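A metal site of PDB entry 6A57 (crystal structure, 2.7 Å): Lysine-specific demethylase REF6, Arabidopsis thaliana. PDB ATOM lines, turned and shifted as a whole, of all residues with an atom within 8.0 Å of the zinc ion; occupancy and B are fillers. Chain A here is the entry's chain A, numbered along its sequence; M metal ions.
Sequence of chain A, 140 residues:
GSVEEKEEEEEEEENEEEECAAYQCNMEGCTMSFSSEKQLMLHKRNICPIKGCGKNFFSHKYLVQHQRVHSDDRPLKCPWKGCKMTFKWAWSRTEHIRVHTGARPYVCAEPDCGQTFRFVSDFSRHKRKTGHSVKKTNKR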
ATOM      1  N   GLN A  24     -21.459  -2.340  -5.498  1.00  0.00           N
ATOM      2  CA  GLN A  24     -21.245  -1.030  -4.860  1.00  0.00           C
ATOM      3  C   GLN A  24     -21.619   0.157  -5.751  1.00  0.00           C
ATOM      4  O   GLN A  24     -21.604   0.047  -6.985  1.00  0.00           O
ATOM      5  CB  GLN A  24     -19.770  -0.901  -4.430  1.00  0.00           C
ATOM      6  CG  GLN A  24     -19.502   0.088  -3.304  1.00  0.00           C
ATOM      7  CD  GLN A  24     -20.099  -0.334  -1.967  1.00  0.00           C
ATOM      8  OE1 GLN A  24     -19.962  -1.489  -1.556  1.00  0.00           O
ATOM      9  N   CYS A  25     -21.985   1.269  -5.119  1.00  0.00           N
ATOM     10  CA  CYS A  25     -22.246   2.554  -5.780  1.00  0.00           C
ATOM     11  C   CYS A  25     -21.142   3.562  -5.466  1.00  0.00           C
ATOM     12  O   CYS A  25     -20.261   3.293  -4.637  1.00  0.00           O
ATOM     13  CB  CYS A  25     -23.605   3.117  -5.327  1.00  0.00           C
ATOM     14  SG  CYS A  25     -24.150   4.619  -6.170  1.00  0.00           S
ATOM     15  N   ASN A  26     -21.209   4.719  -6.105  1.00  0.00           N
ATOM     16  CA  ASN A  26     -20.194   5.778  -5.945  1.00  0.00           C
ATOM     17  C   ASN A  26     -20.853   7.166  -5.880  1.00  0.00           C
ATOM     18  O   ASN A  26     -21.001   7.707  -4.776  1.00  0.00           O
ATOM     19  CB  ASN A  26     -19.118   5.673  -7.042  1.00  0.00           C
ATOM     20  CG  ASN A  26     -19.625   5.040  -8.333  1.00  0.00           C
ATOM     21  OD1 ASN A  26     -20.562   5.543  -8.954  1.00  0.00           O
ATOM     22  ND2 ASN A  26     -19.030   3.926  -8.726  1.00  0.00           N
ATOM     23  N   MET A  27     -21.231   7.729  -7.040  1.00  0.00           N
ATOM     24  CA  MET A  27     -22.022   8.973  -7.120  1.00  0.00           C
ATOM     25  C   MET A  27     -21.553  10.115  -6.215  1.00  0.00           C
ATOM     26  O   MET A  27     -22.363  10.909  -5.732  1.00  0.00           O
ATOM     27  CB  MET A  27     -23.499   8.654  -6.850  1.00  0.00           C
ATOM     28  CG  MET A  27     -24.126   7.647  -7.815  1.00  0.00           C
ATOM     29  SD  MET A  27     -24.426   8.329  -9.452  1.00  0.00           S
ATOM     30  CE  MET A  27     -25.845   9.397  -9.156  1.00  0.00           C
ATOM     31  N   GLU A  28     -20.231  10.219  -6.010  1.00  0.00           N
ATOM     32  CA  GLU A  28     -19.645  11.146  -5.036  1.00  0.00           C
ATOM     33  C   GLU A  28     -20.124  10.859  -3.608  1.00  0.00           C
ATOM     34  O   GLU A  28     -21.025  11.527  -3.095  1.00  0.00           O
ATOM     35  CB  GLU A  28     -19.910  12.601  -5.437  1.00  0.00           C
ATOM     36  N   GLY A  29     -19.532   9.842  -2.982  1.00  0.00           N
ATOM     37  CA  GLY A  29     -19.738   9.568  -1.567  1.00  0.00           C
ATOM     38  C   GLY A  29     -21.003   8.811  -1.183  1.00  0.00           C
ATOM     39  O   GLY A  29     -21.498   8.979  -0.060  1.00  0.00           O
ATOM     40  N   CYS A  30     -21.525   7.973  -2.083  1.00  0.00           N
ATOM     41  CA  CYS A  30     -22.620   7.063  -1.763  1.00  0.00           C
ATOM     42  C   CYS A  30     -22.019   5.734  -1.306  1.00  0.00           C
ATOM     43  O   CYS A  30     -21.540   4.946  -2.128  1.00  0.00           O
ATOM     44  CB  CYS A  30     -23.541   6.873  -2.977  1.00  0.00           C
ATOM     45  SG  CYS A  30     -25.094   5.987  -2.646  1.00  0.00           S
ATOM     46  N   THR A  31     -22.034   5.508   0.015  1.00  0.00           N
ATOM     47  CA  THR A  31     -21.452   4.300   0.622  1.00  0.00           C
ATOM     48  C   THR A  31     -22.539   3.253   0.933  1.00  0.00           C
ATOM     49  O   THR A  31     -22.752   2.890   2.087  1.00  0.00           O
ATOM     50  CB  THR A  31     -20.699   4.661   1.916  1.00  0.00           C
ATOM     51  N   MET A  32     -23.193   2.765  -0.123  1.00  0.00           N
ATOM     52  CA  MET A  32     -24.266   1.771  -0.025  1.00  0.00           C
ATOM     53  C   MET A  32     -24.305   0.892  -1.271  1.00  0.00           C
ATOM     54  O   MET A  32     -24.154   1.394  -2.386  1.00  0.00           O
ATOM     55  CB  MET A  32     -25.622   2.461   0.131  1.00  0.00           C
ATOM     56  N   SER A  33     -24.515  -0.411  -1.087  1.00  0.00           N
ATOM     57  CA  SER A  33     -24.387  -1.406  -2.160  1.00  0.00           C
ATOM     58  C   SER A  33     -25.632  -2.281  -2.318  1.00  0.00           C
ATOM     59  O   SER A  33     -25.965  -3.044  -1.408  1.00  0.00           O
ATOM     60  CB  SER A  33     -23.171  -2.300  -1.900  1.00  0.00           C
ATOM     61  N   LEU A  40     -29.015  -1.725  -8.516  1.00  0.00           N
ATOM     62  CA  LEU A  40     -28.028  -0.634  -8.572  1.00  0.00           C
ATOM     63  C   LEU A  40     -28.224   0.282  -9.798  1.00  0.00           C
ATOM     64  O   LEU A  40     -27.947   1.477  -9.723  1.00  0.00           O
ATOM     65  CB  LEU A  40     -26.594  -1.185  -8.545  1.00  0.00           C
ATOM     66  CG  LEU A  40     -25.460  -0.177  -8.272  1.00  0.00           C
ATOM     67  N   HIS A  43     -31.062   2.523  -8.564  1.00  0.00           N
ATOM     68  CA  HIS A  43     -30.480   3.416  -7.563  1.00  0.00           C
ATOM     69  C   HIS A  43     -29.698   4.552  -8.206  1.00  0.00           C
ATOM     70  O   HIS A  43     -29.884   5.714  -7.847  1.00  0.00           O
ATOM     71  CB  HIS A  43     -29.550   2.636  -6.618  1.00  0.00           C
ATOM     72  CG  HIS A  43     -28.745   3.500  -5.698  1.00  0.00           C
ATOM     73  ND1 HIS A  43     -29.128   3.756  -4.394  1.00  0.00           N
ATOM     74  CD2 HIS A  43     -27.577   4.154  -5.877  1.00  0.00           C
ATOM     75  CE1 HIS A  43     -28.230   4.537  -3.819  1.00  0.00           C
ATOM     76  NE2 HIS A  43     -27.277   4.796  -4.695  1.00  0.00           N
ATOM     77  N   LYS A  44     -28.841   4.197  -9.168  1.00  0.00           N
ATOM     78  CA  LYS A  44     -28.009   5.161  -9.898  1.00  0.00           C
ATOM     79  C   LYS A  44     -28.810   6.291 -10.569  1.00  0.00           C
ATOM     80  O   LYS A  44     -28.333   7.430 -10.617  1.00  0.00           O
ATOM     81  CB  LYS A  44     -27.144   4.439 -10.936  1.00  0.00           C
ATOM     82  N   ARG A  45     -30.013   5.987 -11.047  1.00  0.00           N
ATOM     83  CA  ARG A  45     -30.882   6.983 -11.688  1.00  0.00           C
ATOM     84  C   ARG A  45     -32.000   7.549 -10.781  1.00  0.00           C
ATOM     85  O   ARG A  45     -33.048   7.984 -11.267  1.00  0.00           O
ATOM     86  CB  ARG A  45     -31.445   6.440 -13.016  1.00  0.00           C
ATOM     87  CG  ARG A  45     -32.420   5.280 -12.908  1.00  0.00           C
ATOM     88  CD  ARG A  45     -32.865   4.768 -14.270  1.00  0.00           C
ATOM     89  NE  ARG A  45     -33.680   5.749 -14.988  1.00  0.00           N
ATOM     90  CZ  ARG A  45     -34.491   5.479 -16.019  1.00  0.00           C
ATOM     91  NH1 ARG A  45     -34.640   4.244 -16.481  1.00  0.00           N
ATOM     92  NH2 ARG A  45     -35.174   6.480 -16.582  1.00  0.00           N
ATOM     93  N   ASN A  46     -31.749   7.572  -9.465  1.00  0.00           N
ATOM     94  CA  ASN A  46     -32.654   8.157  -8.452  1.00  0.00           C
ATOM     95  C   ASN A  46     -34.044   7.496  -8.359  1.00  0.00           C
ATOM     96  O   ASN A  46     -35.070   8.174  -8.350  1.00  0.00           O
ATOM     97  CB  ASN A  46     -32.777   9.681  -8.625  1.00  0.00           C
ATOM     98  CG  ASN A  46     -31.476  10.426  -8.334  1.00  0.00           C
ATOM     99  OD1 ASN A  46     -30.441   9.818  -8.061  1.00  0.00           O
ATOM    100  ND2 ASN A  46     -31.545  11.749  -8.389  1.00  0.00           N
ATOM    101  N   HIS A  60     -30.182  12.591  -5.236  1.00  0.00           N
ATOM    102  CA  HIS A  60     -29.587  11.269  -4.954  1.00  0.00           C
ATOM    103  C   HIS A  60     -29.212  11.131  -3.475  1.00  0.00           C
ATOM    104  O   HIS A  60     -29.311  10.034  -2.915  1.00  0.00           O
ATOM    105  CB  HIS A  60     -28.344  11.047  -5.832  1.00  0.00           C
ATOM    106  CG  HIS A  60     -27.801   9.643  -5.801  1.00  0.00           C
ATOM    107  ND1 HIS A  60     -28.228   8.657  -6.666  1.00  0.00           N
ATOM    108  CD2 HIS A  60     -26.855   9.069  -5.016  1.00  0.00           C
ATOM    109  CE1 HIS A  60     -27.581   7.534  -6.410  1.00  0.00           C
ATOM    110  NE2 HIS A  60     -26.735   7.759  -5.415  1.00  0.00           N
ATOM    111  N   LYS A  61     -28.776  12.225  -2.849  1.00  0.00           N
ATOM    112  CA  LYS A  61     -28.413  12.216  -1.433  1.00  0.00           C
ATOM    113  C   LYS A  61     -29.616  11.899  -0.542  1.00  0.00           C
ATOM    114  O   LYS A  61     -29.458  11.269   0.498  1.00  0.00           O
ATOM    115  CB  LYS A  61     -27.795  13.554  -1.010  1.00  0.00           C
ATOM    116  N   LEU A  63     -32.148   9.924  -1.544  1.00  0.00           N
ATOM    117  CA  LEU A  63     -32.392   8.479  -1.774  1.00  0.00           C
ATOM    118  C   LEU A  63     -31.847   7.589  -0.643  1.00  0.00           C
ATOM    119  O   LEU A  63     -32.460   6.606  -0.282  1.00  0.00           O
ATOM    120  CB  LEU A  63     -31.839   8.010  -3.129  1.00  0.00           C
ATOM    121  CG  LEU A  63     -32.726   7.078  -3.956  1.00  0.00           C
ATOM    122  CD1 LEU A  63     -31.976   6.582  -5.187  1.00  0.00           C
ATOM    123  CD2 LEU A  63     -33.255   5.886  -3.164  1.00  0.00           C
ATOM    124  N   VAL A  64     -30.691   7.974  -0.095  1.00  0.00           N
ATOM    125  CA  VAL A  64     -30.120   7.305   1.080  1.00  0.00           C
ATOM    126  C   VAL A  64     -30.938   7.617   2.344  1.00  0.00           C
ATOM    127  O   VAL A  64     -31.192   6.727   3.157  1.00  0.00           O
ATOM    128  CB  VAL A  64     -28.641   7.719   1.289  1.00  0.00           C
ATOM    129  CG1 VAL A  64     -28.098   7.219   2.631  1.00  0.00           C
ATOM    130  CG2 VAL A  64     -27.788   7.193   0.144  1.00  0.00           C
HETATM  131 ZN    ZN M   1     -25.818   6.086  -4.552  1.00  0.00          ZN
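A ring nitrogen (ND1) of His 60 is in hydrogen-bond range of the side-chain amide oxygen (OD1) of Asn 46, 2.9 Å away. O of Met 32 sits close to N of Cys 25, 3.5 Å away.
Residues that only touch the zinc ion: Met 27. Within 4 Å of the zinc ion: Cys 25, Met 27, Cys 30, His 43 and His 60.
The zinc ion is bound by NE2 of His 43, SG of Cys 30, NE2 of His 60 and SG of Cys 25.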
